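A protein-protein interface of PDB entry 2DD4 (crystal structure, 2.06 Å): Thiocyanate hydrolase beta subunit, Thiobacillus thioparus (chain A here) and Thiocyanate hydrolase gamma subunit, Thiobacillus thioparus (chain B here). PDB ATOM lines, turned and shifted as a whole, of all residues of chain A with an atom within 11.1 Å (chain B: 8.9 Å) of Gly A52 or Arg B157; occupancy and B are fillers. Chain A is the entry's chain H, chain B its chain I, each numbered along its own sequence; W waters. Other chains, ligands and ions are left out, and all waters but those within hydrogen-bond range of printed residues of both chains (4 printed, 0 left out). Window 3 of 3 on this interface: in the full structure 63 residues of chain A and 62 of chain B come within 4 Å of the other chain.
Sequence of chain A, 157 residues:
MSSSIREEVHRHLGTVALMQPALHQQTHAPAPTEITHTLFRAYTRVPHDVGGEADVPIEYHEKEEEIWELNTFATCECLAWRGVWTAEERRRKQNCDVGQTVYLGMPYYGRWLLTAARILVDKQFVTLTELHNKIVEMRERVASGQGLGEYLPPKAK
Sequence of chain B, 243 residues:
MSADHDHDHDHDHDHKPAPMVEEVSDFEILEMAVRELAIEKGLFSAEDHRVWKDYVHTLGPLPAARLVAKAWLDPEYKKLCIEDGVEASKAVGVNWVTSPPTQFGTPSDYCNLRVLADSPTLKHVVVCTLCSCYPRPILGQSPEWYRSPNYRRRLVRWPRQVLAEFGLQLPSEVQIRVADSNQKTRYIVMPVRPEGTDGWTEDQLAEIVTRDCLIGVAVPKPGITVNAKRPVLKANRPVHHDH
OD2 of Asp A55 is in salt-bridge range of NH1 of Arg B153 (3.0 Å).
The guanidinium group of Arg B157 is in hydrogen-bond range of the backbone carbonyl oxygen of Gly A52 (2.9 Å).
The backbone carbonyl oxygen (O) of His A48 lies within hydrogen-bond range of the guanidinium group (NH2) of Arg B152, at 3.0 Å.
O of Arg B153 lies within hydrogen-bond range of N of Gly A52, 2.9 Å away.
The backbone carbonyl oxygen (O) of Val A56 sits at hydrogen-bond distance from the side-chain amide nitrogen (ND2) of Asn B150 (2.6 Å).
OH of Tyr A60 sits at hydrogen-bond distance from OD1 of Asn B150 (2.5 Å).
O of His A48 sits close to O of Thr B129 (3.2 Å).
The side-chain carboxylate (OE1) of Glu A53 lies within salt-bridge range of the guanidinium group (NE) of Arg B153, at 2.9 Å.
OH of Tyr A60 sits at hydrogen-bond distance from NH1 of Arg B154 (3.0 Å).
OD1 of Asp A55 lies close to ND2 of Asn B150, 3.3 Å away.
O of Val A56 sits at hydrogen-bond distance from NE of Arg B154.
OE1 of Gln B161 sits close to O of Trp B158 (3.3 Å).
The guanidinium group (NH2) of Arg A45 lies within salt-bridge range of the side-chain carboxylate (OE2) of Glu A53, at 2.7 Å.
The side-chain amide oxygen (OD1) of Asn B150 sits close to the guanidinium group (NH1) of Arg B154 (3.1 Å).
The side-chain hydroxyl (OG1) of Thr B129 is in hydrogen-bond range of the side-chain carboxylate (OD2) of Asp B180, at 2.7 Å.
O of Thr B129 sits at hydrogen-bond distance from NE of Arg B152 (2.8 Å).
Among the printed residues, merely in contact across the chains: Val A50 with Thr B129 (3.6 Å), Val A50 with Arg B152 (3.8 Å), Val A50 with Arg B153 (3.5 Å), Gly A51 with Thr B129 (3.95 Å), Gly A51 with Arg B152 (3.6 Å), Gly A51 with Arg B153 (3.99 Å), Gly A52 with Val B156 (3.7 Å), Glu A53 with Trp B158 (3.8 Å), Ala A54 with Trp B158 (3.7 Å), Asp A55 with Arg B154 (3.8 Å) and Tyr A60 with Tyr B151 (3.4 Å).
Printed residues of chain B within 4 Å of His A48: Thr B129 (3.2 Å) and Arg B152 (3.0 Å).
Of chain B, only Arg B153, Val B156 and Arg B157 come within 4 Å of Gly A52.
Of the printed residues of chain B, Glu A53 touches Arg B153 (2.9 Å) and Trp B158 (3.8 Å).
Printed residues of chain A within 4 Å of Thr B129: His A48 (3.2 Å), Val A50 (3.6 Å) and Gly A51 (3.95 Å).
Val B156 touches one residue of chain A.
Of chain A, only Gly A52 (2.9 Å) comes within 4 Å of Arg B157.
Arg B160 touches none of the printed residues of chain A.
Val B162 touches none of the printed residues of chain A.
The nearest residue of chain B that does not touch Gly A52 is Trp B158 (4.3 Å).
The nearest residue of chain A that does not touch Arg B157 is Glu A53 (5.1 Å).
Of the 12 printed residues of chain A, 9 touch a printed residue of chain B.
Hydrophobic or aromatic side chains of chain A within 4 Å of the printed part of chain B: Val A50 and Tyr A60.
Of the 19 printed residues of chain B, 9 touch a printed residue of chain A.
Hydrophobic or aromatic side chains of chain B that line the printed part of chain A: Tyr B151, Val B156 and Trp B158.
Along chain B the printed residues that touch a printed residue of chain A span positions 129 to 158.
Among the printed residues, 22 pairs touch across the chains.
Water W4 lies within hydrogen-bond range of OD1 of Asp A49 (2.7 Å), OG1 of Thr B129 (2.8 Å), N of Gly A51 (2.8 Å) and N of Val A50 (3.3 Å).
Water W1 lies within hydrogen-bond range of OE1 of Glu A53 (2.8 Å), NH2 of Arg B153 (3.0 Å) and NH1 of Arg A45 (3.2 Å).
Water W3 bridges O of Asp A55 and NH2 of Arg B154.
Water W2 bridges the backbone carbonyl oxygen (O) of Ala A54 (2.8 Å) and the guanidinium group (NH1) of Arg B153 (3.4 Å).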
ATOM      1  N   ARG A  45      10.100   3.120 -11.826  1.00  0.00           N
ATOM      2  CA  ARG A  45       9.654   3.225 -13.214  1.00  0.00           C
ATOM      3  C   ARG A  45       9.749   1.864 -13.898  1.00  0.00           C
ATOM      4  O   ARG A  45      10.477   0.981 -13.447  1.00  0.00           O
ATOM      5  CB  ARG A  45      10.568   4.182 -13.990  1.00  0.00           C
ATOM      6  CG  ARG A  45      11.966   3.572 -14.212  1.00  0.00           C
ATOM      7  CD  ARG A  45      12.871   4.382 -15.134  1.00  0.00           C
ATOM      8  NE  ARG A  45      12.275   4.588 -16.447  1.00  0.00           N
ATOM      9  CZ  ARG A  45      12.929   5.069 -17.499  1.00  0.00           C
ATOM     10  NH1 ARG A  45      14.213   5.389 -17.399  1.00  0.00           N
ATOM     11  NH2 ARG A  45      12.291   5.251 -18.645  1.00  0.00           N
ATOM     12  N   PRO A  47      11.326   0.320 -16.779  1.00  0.00           N
ATOM     13  CA  PRO A  47      12.441   0.596 -17.696  1.00  0.00           C
ATOM     14  C   PRO A  47      12.173   0.779 -19.194  1.00  0.00           C
ATOM     15  O   PRO A  47      12.789   1.637 -19.831  1.00  0.00           O
ATOM     16  CB  PRO A  47      13.402  -0.562 -17.424  1.00  0.00           C
ATOM     17  CG  PRO A  47      13.192  -0.821 -15.970  1.00  0.00           C
ATOM     18  CD  PRO A  47      11.684  -0.770 -15.851  1.00  0.00           C
ATOM     19  N   HIS A  48      11.265  -0.009 -19.762  1.00  0.00           N
ATOM     20  CA  HIS A  48      10.987   0.080 -21.195  1.00  0.00           C
ATOM     21  C   HIS A  48      10.240   1.323 -21.676  1.00  0.00           C
ATOM     22  O   HIS A  48      10.196   1.597 -22.877  1.00  0.00           O
ATOM     23  CB  HIS A  48      10.228  -1.168 -21.659  1.00  0.00           C
ATOM     24  CG  HIS A  48       8.814  -1.244 -21.171  1.00  0.00           C
ATOM     25  ND1 HIS A  48       7.918  -2.182 -21.641  1.00  0.00           N
ATOM     26  CD2 HIS A  48       8.138  -0.502 -20.261  1.00  0.00           C
ATOM     27  CE1 HIS A  48       6.751  -2.012 -21.045  1.00  0.00           C
ATOM     28  NE2 HIS A  48       6.857  -1.000 -20.202  1.00  0.00           N
ATOM     29  N   ASP A  49       9.663   2.074 -20.746  1.00  0.00           N
ATOM     30  CA  ASP A  49       8.887   3.264 -21.090  1.00  0.00           C
ATOM     31  C   ASP A  49       9.786   4.497 -21.257  1.00  0.00           C
ATOM     32  O   ASP A  49       9.885   5.333 -20.358  1.00  0.00           O
ATOM     33  CB  ASP A  49       7.834   3.478 -19.994  1.00  0.00           C
ATOM     34  CG  ASP A  49       6.840   4.565 -20.329  1.00  0.00           C
ATOM     35  OD1 ASP A  49       6.797   5.010 -21.494  1.00  0.00           O
ATOM     36  OD2 ASP A  49       6.087   4.966 -19.415  1.00  0.00           O
ATOM     37  N   VAL A  50      10.427   4.611 -22.420  1.00  0.00           N
ATOM     38  CA  VAL A  50      11.349   5.716 -22.696  1.00  0.00           C
ATOM     39  C   VAL A  50      10.829   6.805 -23.634  1.00  0.00           C
ATOM     40  O   VAL A  50      11.481   7.835 -23.814  1.00  0.00           O
ATOM     41  CB  VAL A  50      12.680   5.192 -23.287  1.00  0.00           C
ATOM     42  CG1 VAL A  50      13.296   4.153 -22.356  1.00  0.00           C
ATOM     43  CG2 VAL A  50      12.438   4.595 -24.675  1.00  0.00           C
ATOM     44  N   GLY A  51       9.665   6.582 -24.235  1.00  0.00           N
ATOM     45  CA  GLY A  51       9.113   7.565 -25.149  1.00  0.00           C
ATOM     46  C   GLY A  51       9.044   8.979 -24.598  1.00  0.00           C
ATOM     47  O   GLY A  51       8.451   9.217 -23.542  1.00  0.00           O
ATOM     48  N   GLY A  52       9.659   9.924 -25.307  1.00  0.00           N
ATOM     49  CA  GLY A  52       9.620  11.309 -24.868  1.00  0.00           C
ATOM     50  C   GLY A  52      10.863  11.809 -24.165  1.00  0.00           C
ATOM     51  O   GLY A  52      11.029  13.018 -23.982  1.00  0.00           O
ATOM     52  N   GLU A  53      11.736  10.892 -23.759  1.00  0.00           N
ATOM     53  CA  GLU A  53      12.973  11.278 -23.088  1.00  0.00           C
ATOM     54  C   GLU A  53      13.876  11.973 -24.101  1.00  0.00           C
ATOM     55  O   GLU A  53      13.941  11.575 -25.261  1.00  0.00           O
ATOM     56  CB  GLU A  53      13.681  10.040 -22.528  1.00  0.00           C
ATOM     57  CG  GLU A  53      12.992   9.408 -21.328  1.00  0.00           C
ATOM     58  CD  GLU A  53      13.626   8.091 -20.929  1.00  0.00           C
ATOM     59  OE1 GLU A  53      14.775   7.831 -21.355  1.00  0.00           O
ATOM     60  OE2 GLU A  53      12.978   7.322 -20.185  1.00  0.00           O
ATOM     61  N   ALA A  54      14.573  13.014 -23.663  1.00  0.00           N
ATOM     62  CA  ALA A  54      15.465  13.744 -24.551  1.00  0.00           C
ATOM     63  C   ALA A  54      16.673  12.882 -24.896  1.00  0.00           C
ATOM     64  O   ALA A  54      17.201  12.172 -24.040  1.00  0.00           O
ATOM     65  CB  ALA A  54      15.916  15.040 -23.885  1.00  0.00           C
ATOM     66  N   ASP A  55      17.093  12.927 -26.155  1.00  0.00           N
ATOM     67  CA  ASP A  55      18.258  12.165 -26.604  1.00  0.00           C
ATOM     68  C   ASP A  55      18.848  12.937 -27.777  1.00  0.00           C
ATOM     69  O   ASP A  55      18.186  13.811 -28.348  1.00  0.00           O
ATOM     70  CB  ASP A  55      17.860  10.751 -27.051  1.00  0.00           C
ATOM     71  CG  ASP A  55      19.036   9.761 -27.006  1.00  0.00           C
ATOM     72  OD1 ASP A  55      20.207  10.192 -27.095  1.00  0.00           O
ATOM     73  OD2 ASP A  55      18.788   8.545 -26.896  1.00  0.00           O
ATOM     74  N   VAL A  56      20.088  12.613 -28.132  1.00  0.00           N
ATOM     75  CA  VAL A  56      20.796  13.291 -29.219  1.00  0.00           C
ATOM     76  C   VAL A  56      20.580  12.629 -30.576  1.00  0.00           C
ATOM     77  O   VAL A  56      20.027  11.533 -30.668  1.00  0.00           O
ATOM     78  CB  VAL A  56      22.319  13.306 -28.953  1.00  0.00           C
ATOM     79  CG1 VAL A  56      22.616  13.937 -27.595  1.00  0.00           C
ATOM     80  CG2 VAL A  56      22.864  11.884 -29.002  1.00  0.00           C
ATOM     81  N   TYR A  60      22.026   6.626 -37.573  1.00  0.00           N
ATOM     82  CA  TYR A  60      21.477   5.278 -37.476  1.00  0.00           C
ATOM     83  C   TYR A  60      22.157   4.280 -38.392  1.00  0.00           C
ATOM     84  O   TYR A  60      22.453   4.574 -39.548  1.00  0.00           O
ATOM     85  CB  TYR A  60      19.976   5.295 -37.768  1.00  0.00           C
ATOM     86  CG  TYR A  60      19.166   6.029 -36.725  1.00  0.00           C
ATOM     87  CD1 TYR A  60      19.194   5.635 -35.385  1.00  0.00           C
ATOM     88  CD2 TYR A  60      18.362   7.111 -37.076  1.00  0.00           C
ATOM     89  CE1 TYR A  60      18.434   6.306 -34.418  1.00  0.00           C
ATOM     90  CE2 TYR A  60      17.599   7.787 -36.121  1.00  0.00           C
ATOM     91  CZ  TYR A  60      17.640   7.380 -34.796  1.00  0.00           C
ATOM     92  OH  TYR A  60      16.889   8.049 -33.852  1.00  0.00           O
ATOM     93  N   VAL B 125       4.439   7.480 -39.700  1.00  0.00           N
ATOM     94  CA  VAL B 125       5.756   6.923 -39.408  1.00  0.00           C
ATOM     95  C   VAL B 125       5.536   6.066 -38.157  1.00  0.00           C
ATOM     96  O   VAL B 125       4.888   6.501 -37.205  1.00  0.00           O
ATOM     97  CB  VAL B 125       6.833   8.022 -39.179  1.00  0.00           C
ATOM     98  CG1 VAL B 125       6.468   8.907 -37.999  1.00  0.00           C
ATOM     99  CG2 VAL B 125       8.200   7.361 -38.975  1.00  0.00           C
ATOM    100  N   VAL B 127       6.696   3.442 -34.862  1.00  0.00           N
ATOM    101  CA  VAL B 127       7.681   3.153 -33.825  1.00  0.00           C
ATOM    102  C   VAL B 127       7.013   2.364 -32.698  1.00  0.00           C
ATOM    103  O   VAL B 127       5.784   2.295 -32.619  1.00  0.00           O
ATOM    104  CB  VAL B 127       8.258   4.464 -33.216  1.00  0.00           C
ATOM    105  CG1 VAL B 127       7.150   5.251 -32.522  1.00  0.00           C
ATOM    106  CG2 VAL B 127       9.370   4.148 -32.225  1.00  0.00           C
ATOM    107  N   THR B 129       7.781   2.588 -28.848  1.00  0.00           N
ATOM    108  CA  THR B 129       8.565   3.162 -27.764  1.00  0.00           C
ATOM    109  C   THR B 129       8.917   2.188 -26.644  1.00  0.00           C
ATOM    110  O   THR B 129       9.975   2.319 -26.025  1.00  0.00           O
ATOM    111  CB  THR B 129       7.862   4.391 -27.141  1.00  0.00           C
ATOM    112  OG1 THR B 129       6.629   3.989 -26.533  1.00  0.00           O
ATOM    113  CG2 THR B 129       7.591   5.445 -28.208  1.00  0.00           C
ATOM    114  N   PRO B 149      17.081   2.680 -28.337  1.00  0.00           N
ATOM    115  CA  PRO B 149      16.438   3.525 -27.329  1.00  0.00           C
ATOM    116  C   PRO B 149      16.300   4.938 -27.907  1.00  0.00           C
ATOM    117  O   PRO B 149      15.333   5.647 -27.640  1.00  0.00           O
ATOM    118  CB  PRO B 149      17.429   3.483 -26.167  1.00  0.00           C
ATOM    119  CG  PRO B 149      17.995   2.099 -26.268  1.00  0.00           C
ATOM    120  CD  PRO B 149      18.216   1.934 -27.756  1.00  0.00           C
ATOM    121  N   ASN B 150      17.283   5.327 -28.713  1.00  0.00           N
ATOM    122  CA  ASN B 150      17.306   6.649 -29.328  1.00  0.00           C
ATOM    123  C   ASN B 150      16.096   6.898 -30.222  1.00  0.00           C
ATOM    124  O   ASN B 150      15.387   7.894 -30.073  1.00  0.00           O
ATOM    125  CB  ASN B 150      18.588   6.816 -30.141  1.00  0.00           C
ATOM    126  CG  ASN B 150      18.725   8.203 -30.718  1.00  0.00           C
ATOM    127  OD1 ASN B 150      18.040   8.559 -31.680  1.00  0.00           O
ATOM    128  ND2 ASN B 150      19.601   9.005 -30.121  1.00  0.00           N
ATOM    129  N   TYR B 151      15.866   5.991 -31.161  1.00  0.00           N
ATOM    130  CA  TYR B 151      14.735   6.115 -32.064  1.00  0.00           C
ATOM    131  C   TYR B 151      13.442   6.077 -31.252  1.00  0.00           C
ATOM    132  O   TYR B 151      12.511   6.844 -31.512  1.00  0.00           O
ATOM    133  CB  TYR B 151      14.760   4.964 -33.072  1.00  0.00           C
ATOM    134  CG  TYR B 151      13.652   4.993 -34.098  1.00  0.00           C
ATOM    135  CD1 TYR B 151      13.652   5.929 -35.135  1.00  0.00           C
ATOM    136  CD2 TYR B 151      12.609   4.067 -34.045  1.00  0.00           C
ATOM    137  CE1 TYR B 151      12.639   5.937 -36.096  1.00  0.00           C
ATOM    138  CE2 TYR B 151      11.599   4.067 -34.997  1.00  0.00           C
ATOM    139  CZ  TYR B 151      11.616   5.000 -36.020  1.00  0.00           C
ATOM    140  OH  TYR B 151      10.616   4.981 -36.969  1.00  0.00           O
ATOM    141  N   ARG B 152      13.407   5.196 -30.252  1.00  0.00           N
ATOM    142  CA  ARG B 152      12.236   5.015 -29.393  1.00  0.00           C
ATOM    143  C   ARG B 152      11.945   6.195 -28.471  1.00  0.00           C
ATOM    144  O   ARG B 152      10.800   6.426 -28.092  1.00  0.00           O
ATOM    145  CB  ARG B 152      12.391   3.724 -28.573  1.00  0.00           C
ATOM    146  CG  ARG B 152      12.339   2.443 -29.424  1.00  0.00           C
ATOM    147  CD  ARG B 152      12.832   1.238 -28.631  1.00  0.00           C
ATOM    148  NE  ARG B 152      12.220   1.210 -27.312  1.00  0.00           N
ATOM    149  CZ  ARG B 152      12.819   0.769 -26.211  1.00  0.00           C
ATOM    150  NH1 ARG B 152      14.063   0.303 -26.267  1.00  0.00           N
ATOM    151  NH2 ARG B 152      12.180   0.819 -25.050  1.00  0.00           N
ATOM    152  N   ARG B 153      12.975   6.945 -28.105  1.00  0.00           N
ATOM    153  CA  ARG B 153      12.775   8.107 -27.246  1.00  0.00           C
ATOM    154  C   ARG B 153      12.322   9.335 -28.040  1.00  0.00           C
ATOM    155  O   ARG B 153      11.396  10.039 -27.640  1.00  0.00           O
ATOM    156  CB  ARG B 153      14.076   8.483 -26.525  1.00  0.00           C
ATOM    157  CG  ARG B 153      14.525   7.552 -25.414  1.00  0.00           C
ATOM    158  CD  ARG B 153      15.909   7.969 -24.911  1.00  0.00           C
ATOM    159  NE  ARG B 153      16.298   7.255 -23.699  1.00  0.00           N
ATOM    160  CZ  ARG B 153      17.506   6.740 -23.492  1.00  0.00           C
ATOM    161  NH1 ARG B 153      18.449   6.859 -24.420  1.00  0.00           N
ATOM    162  NH2 ARG B 153      17.768   6.101 -22.357  1.00  0.00           N
ATOM    163  N   ARG B 154      12.976   9.563 -29.177  1.00  0.00           N
ATOM    164  CA  ARG B 154      12.750  10.750 -29.997  1.00  0.00           C
ATOM    165  C   ARG B 154      11.625  10.849 -31.027  1.00  0.00           C
ATOM    166  O   ARG B 154      11.007  11.902 -31.146  1.00  0.00           O
ATOM    167  CB  ARG B 154      14.049  11.103 -30.721  1.00  0.00           C
ATOM    168  CG  ARG B 154      15.320  10.909 -29.911  1.00  0.00           C
ATOM    169  CD  ARG B 154      16.490  10.729 -30.876  1.00  0.00           C
ATOM    170  NE  ARG B 154      16.720  11.955 -31.614  1.00  0.00           N
ATOM    171  CZ  ARG B 154      17.227  12.037 -32.839  1.00  0.00           C
ATOM    172  NH1 ARG B 154      17.577  10.954 -33.522  1.00  0.00           N
ATOM    173  NH2 ARG B 154      17.372  13.231 -33.382  1.00  0.00           N
ATOM    174  N   LEU B 155      11.376   9.792 -31.793  1.00  0.00           N
ATOM    175  CA  LEU B 155      10.354   9.864 -32.837  1.00  0.00           C
ATOM    176  C   LEU B 155       8.987  10.400 -32.413  1.00  0.00           C
ATOM    177  O   LEU B 155       8.412  11.235 -33.110  1.00  0.00           O
ATOM    178  CB  LEU B 155      10.169   8.501 -33.512  1.00  0.00           C
ATOM    179  CG  LEU B 155       9.287   8.561 -34.767  1.00  0.00           C
ATOM    180  CD1 LEU B 155      10.053   9.252 -35.897  1.00  0.00           C
ATOM    181  CD2 LEU B 155       8.888   7.157 -35.185  1.00  0.00           C
ATOM    182  N   VAL B 156       8.463   9.925 -31.285  1.00  0.00           N
ATOM    183  CA  VAL B 156       7.150  10.372 -30.817  1.00  0.00           C
ATOM    184  C   VAL B 156       7.084  11.857 -30.470  1.00  0.00           C
ATOM    185  O   VAL B 156       6.020  12.471 -30.550  1.00  0.00           O
ATOM    186  CB  VAL B 156       6.674   9.577 -29.565  1.00  0.00           C
ATOM    187  CG1 VAL B 156       6.472   8.113 -29.918  1.00  0.00           C
ATOM    188  CG2 VAL B 156       7.684   9.723 -28.424  1.00  0.00           C
ATOM    189  N   ARG B 157       8.221  12.438 -30.100  1.00  0.00           N
ATOM    190  CA  ARG B 157       8.258  13.842 -29.703  1.00  0.00           C
ATOM    191  C   ARG B 157       8.809  14.813 -30.743  1.00  0.00           C
ATOM    192  O   ARG B 157       8.328  15.941 -30.857  1.00  0.00           O
ATOM    193  CB  ARG B 157       9.055  13.973 -28.405  1.00  0.00           C
ATOM    194  CG  ARG B 157       9.106  15.375 -27.837  1.00  0.00           C
ATOM    195  CD  ARG B 157       9.644  15.343 -26.425  1.00  0.00           C
ATOM    196  NE  ARG B 157       9.364  16.578 -25.709  1.00  0.00           N
ATOM    197  CZ  ARG B 157       9.414  16.691 -24.388  1.00  0.00           C
ATOM    198  NH1 ARG B 157       9.738  15.635 -23.655  1.00  0.00           N
ATOM    199  NH2 ARG B 157       9.121  17.846 -23.801  1.00  0.00           N
ATOM    200  N   TRP B 158       9.820  14.384 -31.491  1.00  0.00           N
ATOM    201  CA  TRP B 158      10.430  15.233 -32.517  1.00  0.00           C
ATOM    202  C   TRP B 158      10.422  14.520 -33.872  1.00  0.00           C
ATOM    203  O   TRP B 158      11.468  14.353 -34.499  1.00  0.00           O
ATOM    204  CB  TRP B 158      11.875  15.570 -32.120  1.00  0.00           C
ATOM    205  CG  TRP B 158      11.997  16.322 -30.812  1.00  0.00           C
ATOM    206  CD1 TRP B 158      11.731  17.645 -30.597  1.00  0.00           C
ATOM    207  CD2 TRP B 158      12.402  15.786 -29.544  1.00  0.00           C
ATOM    208  NE1 TRP B 158      11.947  17.967 -29.276  1.00  0.00           N
ATOM    209  CE2 TRP B 158      12.358  16.844 -28.607  1.00  0.00           C
ATOM    210  CE3 TRP B 158      12.797  14.513 -29.108  1.00  0.00           C
ATOM    211  CZ2 TRP B 158      12.697  16.671 -27.257  1.00  0.00           C
ATOM    212  CZ3 TRP B 158      13.134  14.339 -27.760  1.00  0.00           C
ATOM    213  CH2 TRP B 158      13.080  15.416 -26.854  1.00  0.00           C
ATOM    214  N   PRO B 159       9.238  14.096 -34.345  1.00  0.00           N
ATOM    215  CA  PRO B 159       9.136  13.398 -35.633  1.00  0.00           C
ATOM    216  C   PRO B 159       9.688  14.183 -36.825  1.00  0.00           C
ATOM    217  O   PRO B 159      10.422  13.635 -37.645  1.00  0.00           O
ATOM    218  CB  PRO B 159       7.639  13.116 -35.755  1.00  0.00           C
ATOM    219  CG  PRO B 159       7.024  14.270 -35.022  1.00  0.00           C
ATOM    220  CD  PRO B 159       7.899  14.376 -33.796  1.00  0.00           C
ATOM    221  N   ARG B 160       9.331  15.460 -36.923  1.00  0.00           N
ATOM    222  CA  ARG B 160       9.813  16.303 -38.018  1.00  0.00           C
ATOM    223  C   ARG B 160      11.339  16.257 -38.083  1.00  0.00           C
ATOM    224  O   ARG B 160      11.928  16.065 -39.147  1.00  0.00           O
ATOM    225  CB  ARG B 160       9.378  17.756 -37.801  1.00  0.00           C
ATOM    226  CG  ARG B 160       7.870  17.987 -37.821  1.00  0.00           C
ATOM    227  CD  ARG B 160       7.361  18.114 -39.237  1.00  0.00           C
ATOM    228  NE  ARG B 160       5.906  18.201 -39.302  1.00  0.00           N
ATOM    229  CZ  ARG B 160       5.235  18.455 -40.421  1.00  0.00           C
ATOM    230  NH1 ARG B 160       5.895  18.654 -41.558  1.00  0.00           N
ATOM    231  NH2 ARG B 160       3.911  18.490 -40.413  1.00  0.00           N
ATOM    232  N   GLN B 161      11.970  16.438 -36.928  1.00  0.00           N
ATOM    233  CA  GLN B 161      13.422  16.440 -36.849  1.00  0.00           C
ATOM    234  C   GLN B 161      14.041  15.081 -37.174  1.00  0.00           C
ATOM    235  O   GLN B 161      15.010  15.003 -37.931  1.00  0.00           O
ATOM    236  CB  GLN B 161      13.861  16.928 -35.463  1.00  0.00           C
ATOM    237  CG  GLN B 161      13.441  18.374 -35.175  1.00  0.00           C
ATOM    238  CD  GLN B 161      12.006  18.511 -34.660  1.00  0.00           C
ATOM    239  OE1 GLN B 161      11.195  17.589 -34.768  1.00  0.00           O
ATOM    240  NE2 GLN B 161      11.691  19.678 -34.105  1.00  0.00           N
ATOM    241  N   VAL B 162      13.484  14.011 -36.613  1.00  0.00           N
ATOM    242  CA  VAL B 162      14.001  12.675 -36.881  1.00  0.00           C
ATOM    243  C   VAL B 162      13.822  12.327 -38.358  1.00  0.00           C
ATOM    244  O   VAL B 162      14.734  11.793 -38.986  1.00  0.00           O
ATOM    245  CB  VAL B 162      13.292  11.602 -36.013  1.00  0.00           C
ATOM    246  CG1 VAL B 162      13.718  10.204 -36.455  1.00  0.00           C
ATOM    247  CG2 VAL B 162      13.651  11.809 -34.545  1.00  0.00           C
ATOM    248  N   VAL B 178       2.472   9.958 -35.863  1.00  0.00           N
ATOM    249  CA  VAL B 178       3.374   8.939 -35.356  1.00  0.00           C
ATOM    250  C   VAL B 178       2.501   7.857 -34.732  1.00  0.00           C
ATOM    251  O   VAL B 178       1.651   8.145 -33.888  1.00  0.00           O
ATOM    252  CB  VAL B 178       4.327   9.503 -34.277  1.00  0.00           C
ATOM    253  CG1 VAL B 178       5.183   8.376 -33.700  1.00  0.00           C
ATOM    254  CG2 VAL B 178       5.217  10.595 -34.884  1.00  0.00           C
ATOM    255  N   ASP B 180       2.471   4.654 -32.419  1.00  0.00           N
ATOM    256  CA  ASP B 180       3.256   3.938 -31.416  1.00  0.00           C
ATOM    257  C   ASP B 180       2.573   2.591 -31.154  1.00  0.00           C
ATOM    258  O   ASP B 180       1.560   2.535 -30.450  1.00  0.00           O
ATOM    259  CB  ASP B 180       3.310   4.765 -30.120  1.00  0.00           C
ATOM    260  CG  ASP B 180       4.321   4.229 -29.112  1.00  0.00           C
ATOM    261  OD1 ASP B 180       4.844   3.113 -29.313  1.00  0.00           O
ATOM    262  OD2 ASP B 180       4.586   4.925 -28.105  1.00  0.00           O
HETATM  263  O   HOH W   1      15.888   5.674 -20.059  1.00  0.00           O
HETATM  264  O   HOH W   2      19.062  10.122 -23.744  1.00  0.00           O
HETATM  265  O   HOH W   3      17.909  15.013 -30.826  1.00  0.00           O
HETATM  266  O   HOH W   4       7.583   4.703 -24.053  1.00  0.00           O
